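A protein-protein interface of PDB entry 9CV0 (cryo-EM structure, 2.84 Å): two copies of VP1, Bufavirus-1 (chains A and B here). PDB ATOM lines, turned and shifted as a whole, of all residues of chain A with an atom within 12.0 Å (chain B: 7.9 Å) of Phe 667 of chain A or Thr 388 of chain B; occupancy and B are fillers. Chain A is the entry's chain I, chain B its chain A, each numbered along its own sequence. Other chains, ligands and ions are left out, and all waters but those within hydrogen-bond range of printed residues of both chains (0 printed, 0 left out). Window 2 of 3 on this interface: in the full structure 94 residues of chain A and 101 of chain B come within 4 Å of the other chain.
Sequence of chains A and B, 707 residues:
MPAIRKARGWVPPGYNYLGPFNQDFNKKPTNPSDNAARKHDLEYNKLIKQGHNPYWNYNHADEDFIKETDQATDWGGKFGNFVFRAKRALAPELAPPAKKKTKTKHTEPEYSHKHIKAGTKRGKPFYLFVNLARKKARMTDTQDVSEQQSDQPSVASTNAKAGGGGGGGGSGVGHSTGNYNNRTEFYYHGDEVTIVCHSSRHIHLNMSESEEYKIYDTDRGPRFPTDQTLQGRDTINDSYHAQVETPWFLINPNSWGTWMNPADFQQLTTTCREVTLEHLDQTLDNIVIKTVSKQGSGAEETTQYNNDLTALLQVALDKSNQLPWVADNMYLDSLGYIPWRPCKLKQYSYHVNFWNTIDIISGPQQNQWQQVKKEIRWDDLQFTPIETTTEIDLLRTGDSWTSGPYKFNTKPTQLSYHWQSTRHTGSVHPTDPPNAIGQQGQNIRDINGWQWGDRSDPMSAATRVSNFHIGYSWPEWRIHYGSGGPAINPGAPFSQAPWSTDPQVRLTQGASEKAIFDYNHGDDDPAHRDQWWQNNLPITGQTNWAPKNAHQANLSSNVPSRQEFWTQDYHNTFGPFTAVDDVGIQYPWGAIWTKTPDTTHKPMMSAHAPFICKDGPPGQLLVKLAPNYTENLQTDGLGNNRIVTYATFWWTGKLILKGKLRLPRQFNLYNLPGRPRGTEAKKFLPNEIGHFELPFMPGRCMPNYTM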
ATOM      1  N   LEU A 663       4.281  34.448  28.281  1.00  0.00           N
ATOM      2  CA  LEU A 663       3.146  34.767  27.438  1.00  0.00           C
ATOM      3  C   LEU A 663       2.803  33.563  26.571  1.00  0.00           C
ATOM      4  O   LEU A 663       3.662  32.712  26.332  1.00  0.00           O
ATOM      5  CB  LEU A 663       3.465  35.980  26.559  1.00  0.00           C
ATOM      6  CG  LEU A 663       3.701  37.271  27.339  1.00  0.00           C
ATOM      7  CD1 LEU A 663       4.198  38.358  26.429  1.00  0.00           C
ATOM      8  CD2 LEU A 663       2.433  37.714  28.039  1.00  0.00           C
ATOM      9  N   PRO A 664       1.555  33.439  26.119  1.00  0.00           N
ATOM     10  CA  PRO A 664       1.176  32.255  25.339  1.00  0.00           C
ATOM     11  C   PRO A 664       1.939  32.180  24.025  1.00  0.00           C
ATOM     12  O   PRO A 664       1.970  33.135  23.248  1.00  0.00           O
ATOM     13  CB  PRO A 664      -0.323  32.456  25.108  1.00  0.00           C
ATOM     14  CG  PRO A 664      -0.748  33.361  26.174  1.00  0.00           C
ATOM     15  CD  PRO A 664       0.390  34.287  26.407  1.00  0.00           C
ATOM     16  N   ARG A 665       2.572  31.035  23.791  1.00  0.00           N
ATOM     17  CA  ARG A 665       3.259  30.740  22.542  1.00  0.00           C
ATOM     18  C   ARG A 665       2.452  29.825  21.629  1.00  0.00           C
ATOM     19  O   ARG A 665       2.947  29.390  20.593  1.00  0.00           O
ATOM     20  CB  ARG A 665       4.642  30.159  22.814  1.00  0.00           C
ATOM     21  CG  ARG A 665       5.634  31.204  23.274  1.00  0.00           C
ATOM     22  CD  ARG A 665       6.948  30.588  23.641  1.00  0.00           C
ATOM     23  NE  ARG A 665       7.557  29.867  22.530  1.00  0.00           N
ATOM     24  CZ  ARG A 665       8.312  30.428  21.596  1.00  0.00           C
ATOM     25  NH1 ARG A 665       8.824  29.686  20.628  1.00  0.00           N
ATOM     26  NH2 ARG A 665       8.552  31.729  21.630  1.00  0.00           N
ATOM     27  N   GLN A 666       1.228  29.489  22.010  1.00  0.00           N
ATOM     28  CA  GLN A 666       0.451  28.526  21.250  1.00  0.00           C
ATOM     29  C   GLN A 666      -0.987  29.009  21.162  1.00  0.00           C
ATOM     30  O   GLN A 666      -1.388  29.956  21.837  1.00  0.00           O
ATOM     31  CB  GLN A 666       0.523  27.144  21.890  1.00  0.00           C
ATOM     32  CG  GLN A 666      -0.154  27.078  23.226  1.00  0.00           C
ATOM     33  CD  GLN A 666       0.004  25.745  23.881  1.00  0.00           C
ATOM     34  OE1 GLN A 666       0.949  25.034  23.615  1.00  0.00           O
ATOM     35  NE2 GLN A 666      -0.939  25.384  24.721  1.00  0.00           N
ATOM     36  N   PHE A 667      -1.752  28.362  20.287  1.00  0.00           N
ATOM     37  CA  PHE A 667      -3.181  28.598  20.124  1.00  0.00           C
ATOM     38  C   PHE A 667      -4.003  27.884  21.187  1.00  0.00           C
ATOM     39  O   PHE A 667      -4.888  28.485  21.795  1.00  0.00           O
ATOM     40  CB  PHE A 667      -3.613  28.129  18.735  1.00  0.00           C
ATOM     41  CG  PHE A 667      -5.050  28.405  18.397  1.00  0.00           C
ATOM     42  CD1 PHE A 667      -5.418  29.606  17.840  1.00  0.00           C
ATOM     43  CD2 PHE A 667      -6.024  27.456  18.612  1.00  0.00           C
ATOM     44  CE1 PHE A 667      -6.718  29.851  17.514  1.00  0.00           C
ATOM     45  CE2 PHE A 667      -7.320  27.707  18.291  1.00  0.00           C
ATOM     46  CZ  PHE A 667      -7.667  28.902  17.742  1.00  0.00           C
ATOM     47  N   ASN A 668      -3.718  26.605  21.416  1.00  0.00           N
ATOM     48  CA  ASN A 668      -4.472  25.768  22.333  1.00  0.00           C
ATOM     49  C   ASN A 668      -4.157  26.084  23.792  1.00  0.00           C
ATOM     50  O   ASN A 668      -3.173  26.747  24.121  1.00  0.00           O
ATOM     51  CB  ASN A 668      -4.203  24.293  22.049  1.00  0.00           C
ATOM     52  CG  ASN A 668      -2.737  23.966  22.030  1.00  0.00           C
ATOM     53  OD1 ASN A 668      -1.914  24.819  21.752  1.00  0.00           O
ATOM     54  ND2 ASN A 668      -2.399  22.741  22.379  1.00  0.00           N
ATOM     55  N   LEU A 669      -5.032  25.605  24.670  1.00  0.00           N
ATOM     56  CA  LEU A 669      -4.854  25.761  26.107  1.00  0.00           C
ATOM     57  C   LEU A 669      -3.629  25.016  26.621  1.00  0.00           C
ATOM     58  O   LEU A 669      -3.351  23.890  26.212  1.00  0.00           O
ATOM     59  CB  LEU A 669      -6.087  25.241  26.841  1.00  0.00           C
ATOM     60  CG  LEU A 669      -7.416  25.959  26.707  1.00  0.00           C
ATOM     61  CD1 LEU A 669      -8.468  25.134  27.360  1.00  0.00           C
ATOM     62  CD2 LEU A 669      -7.313  27.271  27.384  1.00  0.00           C
ATOM     63  N   TYR A 670      -2.907  25.652  27.537  1.00  0.00           N
ATOM     64  CA  TYR A 670      -1.876  25.012  28.338  1.00  0.00           C
ATOM     65  C   TYR A 670      -2.478  24.224  29.492  1.00  0.00           C
ATOM     66  O   TYR A 670      -3.616  24.446  29.907  1.00  0.00           O
ATOM     67  CB  TYR A 670      -0.909  26.034  28.920  1.00  0.00           C
ATOM     68  CG  TYR A 670       0.016  26.695  27.944  1.00  0.00           C
ATOM     69  CD1 TYR A 670       1.234  26.124  27.628  1.00  0.00           C
ATOM     70  CD2 TYR A 670      -0.309  27.904  27.368  1.00  0.00           C
ATOM     71  CE1 TYR A 670       2.087  26.727  26.753  1.00  0.00           C
ATOM     72  CE2 TYR A 670       0.539  28.515  26.490  1.00  0.00           C
ATOM     73  CZ  TYR A 670       1.736  27.925  26.185  1.00  0.00           C
ATOM     74  OH  TYR A 670       2.586  28.537  25.305  1.00  0.00           O
ATOM     75  N   ASN A 671      -1.692  23.291  30.013  1.00  0.00           N
ATOM     76  CA  ASN A 671      -1.928  22.731  31.335  1.00  0.00           C
ATOM     77  C   ASN A 671      -1.082  23.519  32.325  1.00  0.00           C
ATOM     78  O   ASN A 671       0.148  23.418  32.314  1.00  0.00           O
ATOM     79  CB  ASN A 671      -1.559  21.253  31.382  1.00  0.00           C
ATOM     80  CG  ASN A 671      -2.417  20.414  30.481  1.00  0.00           C
ATOM     81  OD1 ASN A 671      -3.534  20.784  30.151  1.00  0.00           O
ATOM     82  ND2 ASN A 671      -1.893  19.276  30.064  1.00  0.00           N
ATOM     83  N   LEU A 672      -1.698  24.251  33.126  1.00  0.00           N
ATOM     84  CA  LEU A 672      -1.112  25.193  34.056  1.00  0.00           C
ATOM     85  C   LEU A 672      -0.690  24.510  35.350  1.00  0.00           C
ATOM     86  O   LEU A 672      -1.226  23.461  35.711  1.00  0.00           O
ATOM     87  CB  LEU A 672      -2.109  26.312  34.345  1.00  0.00           C
ATOM     88  CG  LEU A 672      -1.937  27.600  33.545  1.00  0.00           C
ATOM     89  CD1 LEU A 672      -1.807  27.360  32.083  1.00  0.00           C
ATOM     90  CD2 LEU A 672      -3.173  28.389  33.783  1.00  0.00           C
ATOM     91  N   MET A 702       5.478  24.070  32.208  1.00  0.00           N
ATOM     92  CA  MET A 702       4.778  24.104  30.941  1.00  0.00           C
ATOM     93  C   MET A 702       5.755  23.791  29.820  1.00  0.00           C
ATOM     94  O   MET A 702       6.961  24.016  29.959  1.00  0.00           O
ATOM     95  CB  MET A 702       4.164  25.489  30.708  1.00  0.00           C
ATOM     96  CG  MET A 702       3.147  25.929  31.730  1.00  0.00           C
ATOM     97  SD  MET A 702       2.664  27.589  31.293  1.00  0.00           S
ATOM     98  CE  MET A 702       1.671  28.031  32.687  1.00  0.00           C
ATOM     99  N   PRO A 703       5.277  23.252  28.701  1.00  0.00           N
ATOM    100  CA  PRO A 703       6.190  22.863  27.624  1.00  0.00           C
ATOM    101  C   PRO A 703       6.703  24.053  26.836  1.00  0.00           C
ATOM    102  O   PRO A 703       6.135  25.145  26.864  1.00  0.00           O
ATOM    103  CB  PRO A 703       5.321  21.961  26.746  1.00  0.00           C
ATOM    104  CG  PRO A 703       3.970  22.457  26.966  1.00  0.00           C
ATOM    105  CD  PRO A 703       3.896  22.853  28.401  1.00  0.00           C
ATOM    106  N   ASN A 704       7.792  23.822  26.110  1.00  0.00           N
ATOM    107  CA  ASN A 704       8.358  24.845  25.246  1.00  0.00           C
ATOM    108  C   ASN A 704       9.188  24.166  24.167  1.00  0.00           C
ATOM    109  O   ASN A 704       9.596  23.014  24.308  1.00  0.00           O
ATOM    110  CB  ASN A 704       9.192  25.837  26.055  1.00  0.00           C
ATOM    111  CG  ASN A 704       9.425  27.127  25.326  1.00  0.00           C
ATOM    112  OD1 ASN A 704       8.621  27.535  24.499  1.00  0.00           O
ATOM    113  ND2 ASN A 704      10.519  27.792  25.646  1.00  0.00           N
ATOM    114  N   TYR A 705       9.431  24.889  23.080  1.00  0.00           N
ATOM    115  CA  TYR A 705      10.241  24.347  22.000  1.00  0.00           C
ATOM    116  C   TYR A 705      11.722  24.476  22.330  1.00  0.00           C
ATOM    117  O   TYR A 705      12.151  25.448  22.954  1.00  0.00           O
ATOM    118  CB  TYR A 705       9.945  25.066  20.689  1.00  0.00           C
ATOM    119  CG  TYR A 705       8.518  24.970  20.224  1.00  0.00           C
ATOM    120  CD1 TYR A 705       8.057  23.845  19.574  1.00  0.00           C
ATOM    121  CD2 TYR A 705       7.645  26.028  20.395  1.00  0.00           C
ATOM    122  CE1 TYR A 705       6.761  23.761  19.146  1.00  0.00           C
ATOM    123  CE2 TYR A 705       6.349  25.953  19.962  1.00  0.00           C
ATOM    124  CZ  TYR A 705       5.914  24.817  19.337  1.00  0.00           C
ATOM    125  OH  TYR A 705       4.622  24.736  18.902  1.00  0.00           O
ATOM    126  N   TYR B 213      -4.975  23.892   9.020  1.00  0.00           N
ATOM    127  CA  TYR B 213      -3.907  23.236   9.755  1.00  0.00           C
ATOM    128  C   TYR B 213      -4.346  21.825  10.105  1.00  0.00           C
ATOM    129  O   TYR B 213      -5.460  21.622  10.583  1.00  0.00           O
ATOM    130  CB  TYR B 213      -3.590  24.011  11.028  1.00  0.00           C
ATOM    131  CG  TYR B 213      -3.037  25.390  10.801  1.00  0.00           C
ATOM    132  CD1 TYR B 213      -1.681  25.624  10.812  1.00  0.00           C
ATOM    133  CD2 TYR B 213      -3.875  26.451  10.558  1.00  0.00           C
ATOM    134  CE1 TYR B 213      -1.185  26.880  10.612  1.00  0.00           C
ATOM    135  CE2 TYR B 213      -3.388  27.702  10.348  1.00  0.00           C
ATOM    136  CZ  TYR B 213      -2.047  27.913  10.376  1.00  0.00           C
ATOM    137  OH  TYR B 213      -1.574  29.176  10.164  1.00  0.00           O
ATOM    138  N   GLN B 322       9.349  32.940  16.980  1.00  0.00           N
ATOM    139  CA  GLN B 322       8.282  32.369  17.781  1.00  0.00           C
ATOM    140  C   GLN B 322       7.657  31.124  17.174  1.00  0.00           C
ATOM    141  O   GLN B 322       6.898  30.440  17.863  1.00  0.00           O
ATOM    142  CB  GLN B 322       7.205  33.430  18.013  1.00  0.00           C
ATOM    143  CG  GLN B 322       7.700  34.558  18.889  1.00  0.00           C
ATOM    144  CD  GLN B 322       6.748  35.721  18.936  1.00  0.00           C
ATOM    145  OE1 GLN B 322       5.991  35.954  17.999  1.00  0.00           O
ATOM    146  NE2 GLN B 322       6.778  36.463  20.032  1.00  0.00           N
ATOM    147  N   LEU B 323       7.935  30.826  15.976  1.00  0.00           N
ATOM    148  CA  LEU B 323       7.526  29.602  15.308  1.00  0.00           C
ATOM    149  C   LEU B 323       8.601  28.537  15.439  1.00  0.00           C
ATOM    150  O   LEU B 323       9.783  28.867  15.538  1.00  0.00           O
ATOM    151  CB  LEU B 323       7.261  29.856  13.829  1.00  0.00           C
ATOM    152  CG  LEU B 323       6.108  30.769  13.443  1.00  0.00           C
ATOM    153  CD1 LEU B 323       6.177  31.022  11.967  1.00  0.00           C
ATOM    154  CD2 LEU B 323       4.784  30.148  13.807  1.00  0.00           C
ATOM    155  N   TYR B 350       5.922  21.274  10.988  1.00  0.00           N
ATOM    156  CA  TYR B 350       6.792  21.029  12.124  1.00  0.00           C
ATOM    157  C   TYR B 350       6.256  19.874  12.950  1.00  0.00           C
ATOM    158  O   TYR B 350       5.084  19.514  12.867  1.00  0.00           O
ATOM    159  CB  TYR B 350       6.981  22.290  12.976  1.00  0.00           C
ATOM    160  CG  TYR B 350       5.738  22.908  13.556  1.00  0.00           C
ATOM    161  CD1 TYR B 350       5.263  22.526  14.793  1.00  0.00           C
ATOM    162  CD2 TYR B 350       5.061  23.904  12.882  1.00  0.00           C
ATOM    163  CE1 TYR B 350       4.152  23.105  15.333  1.00  0.00           C
ATOM    164  CE2 TYR B 350       3.944  24.481  13.411  1.00  0.00           C
ATOM    165  CZ  TYR B 350       3.493  24.079  14.637  1.00  0.00           C
ATOM    166  OH  TYR B 350       2.371  24.650  15.169  1.00  0.00           O
ATOM    167  N   GLN B 382       1.592  21.060  21.479  1.00  0.00           N
ATOM    168  CA  GLN B 382       1.642  22.485  21.193  1.00  0.00           C
ATOM    169  C   GLN B 382       1.265  22.745  19.744  1.00  0.00           C
ATOM    170  O   GLN B 382       1.832  22.139  18.832  1.00  0.00           O
ATOM    171  CB  GLN B 382       3.030  23.051  21.472  1.00  0.00           C
ATOM    172  CG  GLN B 382       3.315  23.278  22.920  1.00  0.00           C
ATOM    173  CD  GLN B 382       4.690  23.794  23.160  1.00  0.00           C
ATOM    174  OE1 GLN B 382       5.646  23.340  22.560  1.00  0.00           O
ATOM    175  NE2 GLN B 382       4.787  24.828  23.965  1.00  0.00           N
ATOM    176  N   PHE B 383       0.318  23.648  19.536  1.00  0.00           N
ATOM    177  CA  PHE B 383      -0.151  24.019  18.208  1.00  0.00           C
ATOM    178  C   PHE B 383      -0.082  25.531  18.075  1.00  0.00           C
ATOM    179  O   PHE B 383      -0.839  26.253  18.724  1.00  0.00           O
ATOM    180  CB  PHE B 383      -1.562  23.487  17.975  1.00  0.00           C
ATOM    181  CG  PHE B 383      -2.260  24.110  16.817  1.00  0.00           C
ATOM    182  CD1 PHE B 383      -1.833  23.887  15.527  1.00  0.00           C
ATOM    183  CD2 PHE B 383      -3.390  24.878  17.015  1.00  0.00           C
ATOM    184  CE1 PHE B 383      -2.482  24.460  14.469  1.00  0.00           C
ATOM    185  CE2 PHE B 383      -4.047  25.440  15.953  1.00  0.00           C
ATOM    186  CZ  PHE B 383      -3.590  25.228  14.681  1.00  0.00           C
ATOM    187  N   THR B 384       0.832  26.007  17.236  1.00  0.00           N
ATOM    188  CA  THR B 384       0.982  27.431  16.988  1.00  0.00           C
ATOM    189  C   THR B 384       0.724  27.758  15.518  1.00  0.00           C
ATOM    190  O   THR B 384       1.506  27.352  14.648  1.00  0.00           O
ATOM    191  CB  THR B 384       2.373  27.908  17.433  1.00  0.00           C
ATOM    192  OG1 THR B 384       2.571  29.279  17.074  1.00  0.00           O
ATOM    193  CG2 THR B 384       3.470  27.059  16.891  1.00  0.00           C
ATOM    194  N   PRO B 385      -0.376  28.428  15.188  1.00  0.00           N
ATOM    195  CA  PRO B 385      -0.598  28.872  13.814  1.00  0.00           C
ATOM    196  C   PRO B 385       0.253  30.078  13.464  1.00  0.00           C
ATOM    197  O   PRO B 385       0.822  30.753  14.321  1.00  0.00           O
ATOM    198  CB  PRO B 385      -2.084  29.238  13.805  1.00  0.00           C
ATOM    199  CG  PRO B 385      -2.650  28.496  14.902  1.00  0.00           C
ATOM    200  CD  PRO B 385      -1.616  28.509  15.964  1.00  0.00           C
ATOM    201  N   ILE B 386       0.323  30.352  12.166  1.00  0.00           N
ATOM    202  CA  ILE B 386       1.045  31.527  11.704  1.00  0.00           C
ATOM    203  C   ILE B 386       0.241  32.785  11.997  1.00  0.00           C
ATOM    204  O   ILE B 386       0.802  33.855  12.247  1.00  0.00           O
ATOM    205  CB  ILE B 386       1.354  31.400  10.204  1.00  0.00           C
ATOM    206  CG1 ILE B 386       1.930  30.021   9.881  1.00  0.00           C
ATOM    207  CG2 ILE B 386       2.295  32.481   9.765  1.00  0.00           C
ATOM    208  CD1 ILE B 386       3.148  29.665  10.606  1.00  0.00           C
ATOM    209  N   GLU B 387      -1.087  32.669  11.985  1.00  0.00           N
ATOM    210  CA  GLU B 387      -1.955  33.838  12.077  1.00  0.00           C
ATOM    211  C   GLU B 387      -1.940  34.458  13.465  1.00  0.00           C
ATOM    212  O   GLU B 387      -1.911  35.685  13.596  1.00  0.00           O
ATOM    213  CB  GLU B 387      -3.378  33.460  11.681  1.00  0.00           C
ATOM    214  CG  GLU B 387      -3.588  33.263  10.200  1.00  0.00           C
ATOM    215  CD  GLU B 387      -3.141  31.920   9.696  1.00  0.00           C
ATOM    216  OE1 GLU B 387      -2.561  31.145  10.475  1.00  0.00           O
ATOM    217  OE2 GLU B 387      -3.382  31.636   8.507  1.00  0.00           O
ATOM    218  N   THR B 388      -1.980  33.640  14.508  1.00  0.00           N
ATOM    219  CA  THR B 388      -2.010  34.167  15.861  1.00  0.00           C
ATOM    220  C   THR B 388      -0.630  34.513  16.391  1.00  0.00           C
ATOM    221  O   THR B 388      -0.528  35.081  17.480  1.00  0.00           O
ATOM    222  CB  THR B 388      -2.674  33.164  16.800  1.00  0.00           C
ATOM    223  OG1 THR B 388      -1.907  31.957  16.829  1.00  0.00           O
ATOM    224  CG2 THR B 388      -4.081  32.848  16.324  1.00  0.00           C
ATOM    225  N   THR B 389       0.425  34.190  15.652  1.00  0.00           N
ATOM    226  CA  THR B 389       1.801  34.383  16.081  1.00  0.00           C
ATOM    227  C   THR B 389       2.430  35.641  15.500  1.00  0.00           C
ATOM    228  O   THR B 389       2.858  36.519  16.247  1.00  0.00           O
ATOM    229  CB  THR B 389       2.643  33.166  15.694  1.00  0.00           C
ATOM    230  OG1 THR B 389       2.110  31.998  16.320  1.00  0.00           O
ATOM    231  CG2 THR B 389       4.067  33.355  16.138  1.00  0.00           C
ATOM    232  N   THR B 390       2.525  35.727  14.181  1.00  0.00           N
ATOM    233  CA  THR B 390       3.216  36.814  13.512  1.00  0.00           C
ATOM    234  C   THR B 390       2.227  37.614  12.680  1.00  0.00           C
ATOM    235  O   THR B 390       1.153  37.125  12.330  1.00  0.00           O
ATOM    236  CB  THR B 390       4.373  36.273  12.641  1.00  0.00           C
ATOM    237  OG1 THR B 390       5.078  37.356  12.028  1.00  0.00           O
ATOM    238  CG2 THR B 390       3.876  35.327  11.591  1.00  0.00           C
ATOM    239  N   GLU B 391       2.579  38.867  12.404  1.00  0.00           N
ATOM    240  CA  GLU B 391       1.731  39.719  11.584  1.00  0.00           C
ATOM    241  C   GLU B 391       1.970  39.415  10.115  1.00  0.00           C
ATOM    242  O   GLU B 391       3.101  39.152   9.701  1.00  0.00           O
ATOM    243  CB  GLU B 391       2.016  41.188  11.868  1.00  0.00           C
ATOM    244  CG  GLU B 391       1.762  41.587  13.291  1.00  0.00           C
ATOM    245  CD  GLU B 391       2.123  43.025  13.558  1.00  0.00           C
ATOM    246  OE1 GLU B 391       2.626  43.689  12.633  1.00  0.00           O
ATOM    247  OE2 GLU B 391       1.939  43.482  14.704  1.00  0.00           O
ATOM    248  N   ILE B 392       0.912  39.464   9.328  1.00  0.00           N
ATOM    249  CA  ILE B 392       0.927  38.981   7.956  1.00  0.00           C
ATOM    250  C   ILE B 392       0.724  40.155   7.014  1.00  0.00           C
ATOM    251  O   ILE B 392      -0.160  40.987   7.224  1.00  0.00           O
ATOM    252  CB  ILE B 392      -0.156  37.906   7.767  1.00  0.00           C
ATOM    253  CG1 ILE B 392       0.143  36.716   8.672  1.00  0.00           C
ATOM    254  CG2 ILE B 392      -0.232  37.468   6.340  1.00  0.00           C
ATOM    255  CD1 ILE B 392      -0.986  35.747   8.800  1.00  0.00           C
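The backbone carbonyl oxygen (O) of Gln 322 of chain B sits at hydrogen-bond distance from the guanidinium group (NH1) of Arg 665 of chain A, at 3.5 Å. NE2 of Gln 382 of chain B sits at hydrogen-bond distance from O of Pro 703 of chain A, 3.2 Å away. O of Phe 383 of chain B is in hydrogen-bond range of N of Phe 667 of chain A, 2.8 Å away. The side-chain amide oxygen (OD1) of Asn 668 of chain A lies within hydrogen-bond range of the backbone NH (N) of Phe 383 of chain B, at 3.4 Å.
The backbone carbonyl oxygen (O) of Thr 384 of chain B is in hydrogen-bond range of the side-chain hydroxyl (OH) of Tyr 350 of chain B. O of Pro 385 of chain B is in hydrogen-bond range of OG1 of Thr 389 of chain B (2.7 Å). The backbone NH (N) of Arg 665 of chain A is in hydrogen-bond range of the side-chain hydroxyl (OH) of Tyr 670 of chain A. The side-chain amide nitrogen (NE2) of Gln 666 of chain A sits at hydrogen-bond distance from the backbone carbonyl oxygen (O) of Asn 668 of chain A, 2.7 Å away. The side-chain amide nitrogen (NE2) of Gln 666 of chain A sits at hydrogen-bond distance from the backbone carbonyl oxygen (O) of Leu 669 of chain A (3.2 Å). The backbone NH of Tyr 670 of chain A lies close to the side-chain amide nitrogen of Gln 666 of chain A.
Among the printed residues, merely in contact across the chains: Arg 665 of chain A with Thr 384 of chain B (3.5 Å), Gln 666 of chain A with Gln 382 of chain B (3.0 Å), Gln 666 of chain A with Phe 383 of chain B (3.6 Å), Phe 667 of chain A with Pro 385 of chain B (3.4 Å), Phe 667 of chain A with Thr 388 of chain B (3.8 Å), Asn 704 of chain A with Gln 382 of chain B (3.8 Å), Tyr 705 of chain A with Tyr 350 of chain B (3.95 Å), Tyr 705 of chain A with Gln 382 of chain B (3.5 Å) and Tyr 705 of chain A with Thr 384 of chain B (3.3 Å).
Of the printed residues of chain A, Thr 388 of chain B touches Phe 667. Of chain A, only Gln 666 (3.6 Å), Phe 667 (2.8 Å) and Asn 668 (3.4 Å) come within 4 Å of Phe 383 of chain B. Thr 384 of chain B touches just these residues of chain A: Arg 665 (3.5 Å) and Tyr 705 (3.3 Å). No residue of chain A comes within 4 Å of Ile 386 of chain B. No residue of chain A comes within 4 Å of Glu 387 of chain B. No residue of chain A comes within 4 Å of Thr 390 of chain B. Printed residues of chain B within 4 Å of Pro 703 of chain A: Gln 382 (3.2 Å). Of the printed residues of chain B, Asn 668 of chain A touches Phe 383. Met 702 of chain A touches none of the printed residues of chain B. Tyr 670 of chain A touches none of the printed residues of chain B. The nearest residue of chain B that does not touch Phe 667 of chain A is Thr 384 of chain B (4.4 Å).
Of the 14 printed residues of chain A, 7 touch a printed residue of chain B. Hydrophobic or aromatic side chains of chain A that line the printed part of chain B: Phe 667, Pro 703 and Tyr 705. Of the 15 printed residues of chain B, 7 touch a printed residue of chain A. Printed residues of chain B that touch a printed residue of chain A: Gln 322, Tyr 350, Gln 382, Phe 383, Thr 384, Pro 385 and Thr 388. Hydrophobic or aromatic side chains of chain B that line the printed part of chain A: Tyr 350, Phe 383 and Pro 385. Among the printed residues, no Asp or Glu carboxylate lies within 4 Å of a Lys or Arg side-chain nitrogen of the other chain.
No position is printed for both chains. Of the 13 pairs that touch across the chains among the printed residues, none has its exchanged pair printed and touching as well.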
